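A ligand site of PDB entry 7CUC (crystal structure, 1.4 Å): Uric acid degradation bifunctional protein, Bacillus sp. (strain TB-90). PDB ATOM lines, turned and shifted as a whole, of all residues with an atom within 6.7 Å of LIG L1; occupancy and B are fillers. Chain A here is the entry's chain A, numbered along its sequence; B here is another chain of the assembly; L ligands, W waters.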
ATOM      1  N   SER A 177      15.778   3.017 -22.694  1.00  0.00           N
ATOM      2  CA  SER A 177      15.509   1.678 -22.202  1.00  0.00           C
ATOM      3  C   SER A 177      15.081   1.734 -20.745  1.00  0.00           C
ATOM      4  O   SER A 177      15.320   2.716 -20.012  1.00  0.00           O
ATOM      5  CB  SER A 177      16.735   0.747 -22.320  1.00  0.00           C
ATOM      6  OG  SER A 177      17.716   1.025 -21.328  1.00  0.00           O
ATOM      7  N   PHE A 178      14.391   0.672 -20.319  1.00  0.00           N
ATOM      8  CA  PHE A 178      14.147   0.427 -18.900  1.00  0.00           C
ATOM      9  C   PHE A 178      14.247  -1.087 -18.715  1.00  0.00           C
ATOM     10  O   PHE A 178      13.287  -1.809 -19.005  1.00  0.00           O
ATOM     11  CB  PHE A 178      12.811   0.967 -18.420  1.00  0.00           C
ATOM     12  CG  PHE A 178      12.664   0.912 -16.926  1.00  0.00           C
ATOM     13  CD1 PHE A 178      13.582   1.536 -16.086  1.00  0.00           C
ATOM     14  CD2 PHE A 178      11.636   0.216 -16.350  1.00  0.00           C
ATOM     15  CE1 PHE A 178      13.451   1.481 -14.715  1.00  0.00           C
ATOM     16  CE2 PHE A 178      11.505   0.146 -14.970  1.00  0.00           C
ATOM     17  CZ  PHE A 178      12.410   0.771 -14.160  1.00  0.00           C
ATOM     18  N   PHE A 181      15.480  -3.977 -13.724  1.00  0.00           N
ATOM     19  CA  PHE A 181      14.785  -3.719 -12.465  1.00  0.00           C
ATOM     20  C   PHE A 181      14.358  -5.049 -11.815  1.00  0.00           C
ATOM     21  O   PHE A 181      14.403  -6.117 -12.416  1.00  0.00           O
ATOM     22  CB  PHE A 181      13.608  -2.771 -12.710  1.00  0.00           C
ATOM     23  CG  PHE A 181      12.688  -3.225 -13.816  1.00  0.00           C
ATOM     24  CD1 PHE A 181      11.629  -4.074 -13.521  1.00  0.00           C
ATOM     25  CD2 PHE A 181      12.880  -2.827 -15.139  1.00  0.00           C
ATOM     26  CE1 PHE A 181      10.778  -4.531 -14.536  1.00  0.00           C
ATOM     27  CE2 PHE A 181      12.014  -3.261 -16.159  1.00  0.00           C
ATOM     28  CZ  PHE A 181      10.964  -4.146 -15.857  1.00  0.00           C
ATOM     29  N   LEU A 189       5.827  -5.983 -15.421  1.00  0.00           N
ATOM     30  CA  LEU A 189       6.267  -5.070 -16.467  1.00  0.00           C
ATOM     31  C   LEU A 189       7.333  -5.725 -17.320  1.00  0.00           C
ATOM     32  O   LEU A 189       8.340  -6.182 -16.770  1.00  0.00           O
ATOM     33  CB  LEU A 189       6.879  -3.844 -15.797  1.00  0.00           C
ATOM     34  CG  LEU A 189       7.363  -2.722 -16.691  1.00  0.00           C
ATOM     35  CD1 LEU A 189       6.199  -2.147 -17.483  1.00  0.00           C
ATOM     36  CD2 LEU A 189       8.070  -1.609 -15.924  1.00  0.00           C
ATOM     37  N   ARG A 195      11.945   2.184 -25.652  1.00  0.00           N
ATOM     38  CA  ARG A 195      10.601   2.683 -25.407  1.00  0.00           C
ATOM     39  C   ARG A 195      10.508   4.146 -25.798  1.00  0.00           C
ATOM     40  O   ARG A 195      11.517   4.863 -25.819  1.00  0.00           O
ATOM     41  CB  ARG A 195      10.210   2.536 -23.930  1.00  0.00           C
ATOM     42  CG  ARG A 195      11.128   3.272 -22.971  1.00  0.00           C
ATOM     43  CD  ARG A 195      10.697   3.088 -21.541  1.00  0.00           C
ATOM     44  NE  ARG A 195      11.521   3.887 -20.640  1.00  0.00           N
ATOM     45  CZ  ARG A 195      11.327   4.009 -19.331  1.00  0.00           C
ATOM     46  NH1 ARG A 195      10.309   3.401 -18.732  1.00  0.00           N
ATOM     47  NH2 ARG A 195      12.135   4.781 -18.620  1.00  0.00           N
ATOM     48  N   LEU A 197       9.865   7.121 -24.357  1.00  0.00           N
ATOM     49  CA  LEU A 197       9.687   7.646 -23.021  1.00  0.00           C
ATOM     50  C   LEU A 197       9.012   9.006 -23.072  1.00  0.00           C
ATOM     51  O   LEU A 197       9.473   9.924 -23.776  1.00  0.00           O
ATOM     52  CB  LEU A 197      11.049   7.764 -22.345  1.00  0.00           C
ATOM     53  CG  LEU A 197      11.072   8.387 -20.958  1.00  0.00           C
ATOM     54  CD1 LEU A 197      10.166   7.652 -20.028  1.00  0.00           C
ATOM     55  CD2 LEU A 197      12.506   8.376 -20.454  1.00  0.00           C
ATOM     56  N   LEU A 241      18.403   5.387 -19.425  1.00  0.00           N
ATOM     57  CA  LEU A 241      18.286   4.086 -18.778  1.00  0.00           C
ATOM     58  C   LEU A 241      17.129   4.028 -17.779  1.00  0.00           C
ATOM     59  O   LEU A 241      16.855   2.944 -17.247  1.00  0.00           O
ATOM     60  CB  LEU A 241      19.597   3.735 -18.059  1.00  0.00           C
ATOM     61  CG  LEU A 241      20.851   3.635 -18.933  1.00  0.00           C
ATOM     62  CD1 LEU A 241      22.132   3.592 -18.096  1.00  0.00           C
ATOM     63  CD2 LEU A 241      20.811   2.399 -19.838  1.00  0.00           C
ATOM     64  N   SER A 242      16.506   5.167 -17.487  1.00  0.00           N
ATOM     65  CA  SER A 242      15.348   5.349 -16.638  1.00  0.00           C
ATOM     66  C   SER A 242      15.131   6.860 -16.578  1.00  0.00           C
ATOM     67  O   SER A 242      16.003   7.635 -16.974  1.00  0.00           O
ATOM     68  CB  SER A 242      15.576   4.849 -15.229  1.00  0.00           C
ATOM     69  OG  SER A 242      16.607   5.597 -14.612  1.00  0.00           O
ATOM     70  N   ILE A 243      13.970   7.264 -16.065  1.00  0.00           N
ATOM     71  CA  ILE A 243      13.773   8.689 -15.803  1.00  0.00           C
ATOM     72  C   ILE A 243      14.750   9.177 -14.743  1.00  0.00           C
ATOM     73  O   ILE A 243      15.283  10.291 -14.831  1.00  0.00           O
ATOM     74  CB  ILE A 243      12.316   8.981 -15.423  1.00  0.00           C
ATOM     75  CG1 ILE A 243      11.388   8.721 -16.599  1.00  0.00           C
ATOM     76  CG2 ILE A 243      12.157  10.444 -14.990  1.00  0.00           C
ATOM     77  CD1 ILE A 243       9.895   8.683 -16.216  1.00  0.00           C
ATOM     78  N   GLN A 244      14.971   8.372 -13.712  1.00  0.00           N
ATOM     79  CA  GLN A 244      15.940   8.729 -12.679  1.00  0.00           C
ATOM     80  C   GLN A 244      17.293   9.126 -13.277  1.00  0.00           C
ATOM     81  O   GLN A 244      17.884  10.157 -12.916  1.00  0.00           O
ATOM     82  CB  GLN A 244      16.081   7.525 -11.744  1.00  0.00           C
ATOM     83  CG  GLN A 244      14.854   7.203 -10.874  1.00  0.00           C
ATOM     84  CD  GLN A 244      13.885   6.192 -11.505  1.00  0.00           C
ATOM     85  OE1 GLN A 244      13.595   6.222 -12.694  1.00  0.00           O
ATOM     86  NE2 GLN A 244      13.349   5.299 -10.667  1.00  0.00           N
ATOM     87  N   ASN A 270       6.086   9.720 -15.299  1.00  0.00           N
ATOM     88  CA  ASN A 270       6.148   8.842 -16.465  1.00  0.00           C
ATOM     89  C   ASN A 270       4.751   8.680 -17.044  1.00  0.00           C
ATOM     90  O   ASN A 270       3.839   8.188 -16.348  1.00  0.00           O
ATOM     91  CB  ASN A 270       6.668   7.471 -16.056  1.00  0.00           C
ATOM     92  CG  ASN A 270       7.035   6.606 -17.239  1.00  0.00           C
ATOM     93  OD1 ASN A 270       6.629   6.847 -18.375  1.00  0.00           O
ATOM     94  ND2 ASN A 270       7.799   5.559 -16.968  1.00  0.00           N
ATOM     95  N   GLY A 296       4.035   6.655 -12.805  1.00  0.00           N
ATOM     96  CA  GLY A 296       5.228   6.695 -11.993  1.00  0.00           C
ATOM     97  C   GLY A 296       5.705   8.129 -11.796  1.00  0.00           C
ATOM     98  O   GLY A 296       5.455   9.021 -12.628  1.00  0.00           O
ATOM     99  N   PHE A 297       6.416   8.374 -10.711  1.00  0.00           N
ATOM    100  CA  PHE A 297       7.019   9.675 -10.518  1.00  0.00           C
ATOM    101  C   PHE A 297       8.334   9.540  -9.766  1.00  0.00           C
ATOM    102  O   PHE A 297       8.592   8.541  -9.089  1.00  0.00           O
ATOM    103  CB  PHE A 297       6.062  10.657  -9.778  1.00  0.00           C
ATOM    104  CG  PHE A 297       5.693  10.210  -8.361  1.00  0.00           C
ATOM    105  CD1 PHE A 297       6.531  10.471  -7.300  1.00  0.00           C
ATOM    106  CD2 PHE A 297       4.507   9.549  -8.116  1.00  0.00           C
ATOM    107  CE1 PHE A 297       6.205  10.044  -5.998  1.00  0.00           C
ATOM    108  CE2 PHE A 297       4.180   9.140  -6.806  1.00  0.00           C
ATOM    109  CZ  PHE A 297       5.040   9.387  -5.759  1.00  0.00           C
ATOM    110  N   GLN A 298       9.161  10.578  -9.895  1.00  0.00           N
ATOM    111  CA  GLN A 298      10.492  10.637  -9.314  1.00  0.00           C
ATOM    112  C   GLN A 298      10.702  12.053  -8.778  1.00  0.00           C
ATOM    113  O   GLN A 298      10.196  13.008  -9.359  1.00  0.00           O
ATOM    114  CB  GLN A 298      11.574  10.352 -10.361  1.00  0.00           C
ATOM    115  CG  GLN A 298      11.512   8.983 -10.961  1.00  0.00           C
ATOM    116  CD  GLN A 298      10.422   8.814 -11.990  1.00  0.00           C
ATOM    117  OE1 GLN A 298       9.974   9.770 -12.617  1.00  0.00           O
ATOM    118  NE2 GLN A 298      10.014   7.564 -12.177  1.00  0.00           N
ATOM    119  N   TYR B   5      10.812   8.107  -5.115  1.00  0.00           N
ATOM    120  CA  TYR B   5      10.071   7.802  -6.342  1.00  0.00           C
ATOM    121  C   TYR B   5       8.869   6.977  -5.944  1.00  0.00           C
ATOM    122  O   TYR B   5       8.783   6.484  -4.817  1.00  0.00           O
ATOM    123  CB  TYR B   5      10.991   7.182  -7.418  1.00  0.00           C
ATOM    124  CG  TYR B   5      11.216   5.718  -7.258  1.00  0.00           C
ATOM    125  CD1 TYR B   5      11.890   5.198  -6.150  1.00  0.00           C
ATOM    126  CD2 TYR B   5      10.815   4.852  -8.257  1.00  0.00           C
ATOM    127  CE1 TYR B   5      12.096   3.858  -6.029  1.00  0.00           C
ATOM    128  CE2 TYR B   5      11.028   3.506  -8.146  1.00  0.00           C
ATOM    129  CZ  TYR B   5      11.659   3.008  -7.044  1.00  0.00           C
ATOM    130  OH  TYR B   5      11.852   1.644  -6.917  1.00  0.00           O
ATOM    131  N   GLY B   6       7.900   6.871  -6.853  1.00  0.00           N
ATOM    132  CA  GLY B   6       6.712   6.083  -6.564  1.00  0.00           C
ATOM    133  C   GLY B   6       5.665   6.083  -7.650  1.00  0.00           C
ATOM    134  O   GLY B   6       5.957   6.241  -8.838  1.00  0.00           O
ATOM    135  N   LYS B   7       4.427   5.867  -7.228  1.00  0.00           N
ATOM    136  CA  LYS B   7       3.326   5.730  -8.158  1.00  0.00           C
ATOM    137  C   LYS B   7       2.127   6.513  -7.643  1.00  0.00           C
ATOM    138  O   LYS B   7       1.788   6.443  -6.464  1.00  0.00           O
ATOM    139  CB  LYS B   7       2.954   4.262  -8.239  1.00  0.00           C
ATOM    140  CG  LYS B   7       2.131   3.902  -9.474  1.00  0.00           C
ATOM    141  CD  LYS B   7       3.003   3.782 -10.704  1.00  0.00           C
ATOM    142  CE  LYS B   7       2.299   3.112 -11.865  1.00  0.00           C
ATOM    143  NZ  LYS B   7       3.281   3.025 -13.004  1.00  0.00           N
ATOM    144  N   ASN B  61      19.512  -0.076 -12.311  1.00  0.00           N
ATOM    145  CA  ASN B  61      18.176  -0.457 -11.922  1.00  0.00           C
ATOM    146  C   ASN B  61      18.140  -1.657 -10.993  1.00  0.00           C
ATOM    147  O   ASN B  61      17.040  -2.080 -10.630  1.00  0.00           O
ATOM    148  CB  ASN B  61      17.304  -0.663 -13.168  1.00  0.00           C
ATOM    149  CG  ASN B  61      17.040   0.649 -13.887  1.00  0.00           C
ATOM    150  OD1 ASN B  61      16.818   1.684 -13.231  1.00  0.00           O
ATOM    151  ND2 ASN B  61      17.045   0.633 -15.211  1.00  0.00           N
ATOM    152  N   VAL B  64      15.845  -1.169  -8.094  1.00  0.00           N
ATOM    153  CA  VAL B  64      14.616  -0.455  -8.433  1.00  0.00           C
ATOM    154  C   VAL B  64      13.449  -1.411  -8.485  1.00  0.00           C
ATOM    155  O   VAL B  64      13.386  -2.308  -9.343  1.00  0.00           O
ATOM    156  CB  VAL B  64      14.757   0.302  -9.762  1.00  0.00           C
ATOM    157  CG1 VAL B  64      13.433   0.959 -10.156  1.00  0.00           C
ATOM    158  CG2 VAL B  64      15.812   1.385  -9.663  1.00  0.00           C
ATOM    159  N   VAL B  65      12.510  -1.226  -7.566  1.00  0.00           N
ATOM    160  CA  VAL B  65      11.186  -1.816  -7.675  1.00  0.00           C
ATOM    161  C   VAL B  65      10.454  -0.977  -8.722  1.00  0.00           C
ATOM    162  O   VAL B  65      10.277   0.226  -8.549  1.00  0.00           O
ATOM    163  CB  VAL B  65      10.448  -1.753  -6.323  1.00  0.00           C
ATOM    164  CG1 VAL B  65       9.054  -2.326  -6.456  1.00  0.00           C
ATOM    165  CG2 VAL B  65      11.218  -2.505  -5.223  1.00  0.00           C
ATOM    166  N   ALA B  66      10.057  -1.580  -9.823  1.00  0.00           N
ATOM    167  CA  ALA B  66       9.348  -0.801 -10.827  1.00  0.00           C
ATOM    168  C   ALA B  66       8.111  -0.150 -10.215  1.00  0.00           C
ATOM    169  O   ALA B  66       7.426  -0.730  -9.388  1.00  0.00           O
ATOM    170  CB  ALA B  66       8.987  -1.698 -12.002  1.00  0.00           C
ATOM    171  N   THR B  67       7.810   1.067 -10.644  1.00  0.00           N
ATOM    172  CA  THR B  67       6.596   1.695 -10.127  1.00  0.00           C
ATOM    173  C   THR B  67       5.359   0.879 -10.488  1.00  0.00           C
ATOM    174  O   THR B  67       4.397   0.829  -9.709  1.00  0.00           O
ATOM    175  CB  THR B  67       6.476   3.155 -10.566  1.00  0.00           C
ATOM    176  OG1 THR B  67       6.239   3.228 -11.975  1.00  0.00           O
ATOM    177  CG2 THR B  67       7.739   3.892 -10.200  1.00  0.00           C
ATOM    178  N   ASP B  68       5.376   0.220 -11.659  1.00  0.00           N
ATOM    179  CA  ASP B  68       4.269  -0.654 -12.045  1.00  0.00           C
ATOM    180  C   ASP B  68       4.093  -1.770 -11.026  1.00  0.00           C
ATOM    181  O   ASP B  68       2.958  -2.169 -10.722  1.00  0.00           O
ATOM    182  CB  ASP B  68       4.578  -1.265 -13.419  1.00  0.00           C
ATOM    183  CG  ASP B  68       3.450  -2.069 -13.968  1.00  0.00           C
ATOM    184  OD1 ASP B  68       2.549  -1.449 -14.555  1.00  0.00           O
ATOM    185  OD2 ASP B  68       3.446  -3.318 -13.830  1.00  0.00           O
ATOM    186  N   SER B  69       5.189  -2.293 -10.489  1.00  0.00           N
ATOM    187  CA  SER B  69       5.087  -3.318  -9.469  1.00  0.00           C
ATOM    188  C   SER B  69       4.513  -2.775  -8.171  1.00  0.00           C
ATOM    189  O   SER B  69       3.810  -3.514  -7.458  1.00  0.00           O
ATOM    190  CB  SER B  69       6.455  -3.935  -9.211  1.00  0.00           C
ATOM    191  OG  SER B  69       7.015  -4.352 -10.447  1.00  0.00           O
ATOM    192  N   MET B  70       4.762  -1.498  -7.865  1.00  0.00           N
ATOM    193  CA  MET B  70       4.167  -0.915  -6.665  1.00  0.00           C
ATOM    194  C   MET B  70       2.638  -0.851  -6.823  1.00  0.00           C
ATOM    195  O   MET B  70       1.892  -1.079  -5.859  1.00  0.00           O
ATOM    196  CB  MET B  70       4.657   0.502  -6.398  1.00  0.00           C
ATOM    197  CG  MET B  70       6.150   0.573  -6.151  1.00  0.00           C
ATOM    198  SD  MET B  70       6.694   2.277  -6.015  1.00  0.00           S
ATOM    199  CE  MET B  70       8.448   2.007  -6.007  1.00  0.00           C
HETATM  200  N1  LIG L   1      11.599   4.509 -13.822  1.00  0.00           N
HETATM  201  C1  LIG L   1      11.384   4.540 -15.180  1.00  0.00           C
HETATM  202  O1  LIG L   1      12.039   5.249 -15.882  1.00  0.00           O
HETATM  203  N2  LIG L   1      10.424   3.763 -15.748  1.00  0.00           N
HETATM  204  C2  LIG L   1       9.708   2.966 -14.952  1.00  0.00           C
HETATM  205  C3  LIG L   1       9.925   2.908 -13.606  1.00  0.00           C
HETATM  206  C4  LIG L   1      10.897   3.709 -13.043  1.00  0.00           C
HETATM  207  O2  LIG L   1      11.086   3.708 -11.857  1.00  0.00           O
HETATM  208  N3  LIG L   1       9.047   2.023 -13.080  1.00  0.00           N
HETATM  209  N4  LIG L   1       8.304   1.531 -14.103  1.00  0.00           N
HETATM  210  N5  LIG L   1       8.719   2.104 -15.249  1.00  0.00           N
HETATM  211  O1  LG2 L   2       7.410   4.900 -13.755  1.00  0.00           O
HETATM  212  O2  LG2 L   2       8.351   5.664 -13.639  1.00  0.00           O
HETATM  213  O   HOH W   1       7.517   1.736 -17.697  1.00  0.00           O
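Water W1 bridges a nitrogen (N5) of LIG L1 (2.8 Å) and the guanidinium group (NH1) of Arg 195 (3.4 Å).
A nitrogen (N1) of LIG L1 lies close to an oxygen (O2) of LG2 L2 (3.5 Å).
The side-chain hydroxyl (OG1) of Thr 67 of chain B sits at hydrogen-bond distance from the side-chain amino group (NZ) of Lys 7 of chain B.
The backbone carbonyl oxygen (O) of Gly 296 is in hydrogen-bond range of the backbone NH (N) of Asn 270 (2.8 Å).
The backbone carbonyl oxygen of Val 65 of chain B lies within hydrogen-bond range of the side-chain hydroxyl of Tyr 5 of chain B (2.7 Å).
The backbone NH of Gln 244 sits close to the side-chain hydroxyl of Ser 242, 3.3 Å away.
Residues that only touch LIG L1: Phe 178, Leu 189, Ser 242, Gln 298, Tyr 5 of chain B, Val 64 of chain B and Ala 66 of chain B.
An oxygen (O2) of LG2 L2 is in hydrogen-bond range of the side-chain amide nitrogen (NE2) of Gln 298 (2.9 Å).
The backbone NH (N) of Ile 243 lies within hydrogen-bond range of an oxygen (O1) of LIG L1 (2.8 Å).
A nitrogen (N2) of LIG L1 lies close to the side-chain amide nitrogen of Asn 270, 3.4 Å away.
OG1 of Thr 67 of chain B is in hydrogen-bond range of N3 of LIG L1 (3.2 Å).
N of Thr 67 of chain B is in hydrogen-bond range of N3 of LIG L1 (2.9 Å).
An oxygen (O1) of LG2 L2 is in hydrogen-bond range of the side-chain hydroxyl of Thr 67 of chain B (2.7 Å).
NH2 of Arg 195 is in hydrogen-bond range of O1 of LIG L1.
The side-chain amide nitrogen (ND2) of Asn 270 sits at hydrogen-bond distance from an oxygen (O1) of LG2 L2, at 3.3 Å.
The side-chain amide oxygen of Gln 244 sits at hydrogen-bond distance from a nitrogen (N1) of LIG L1 (2.9 Å).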
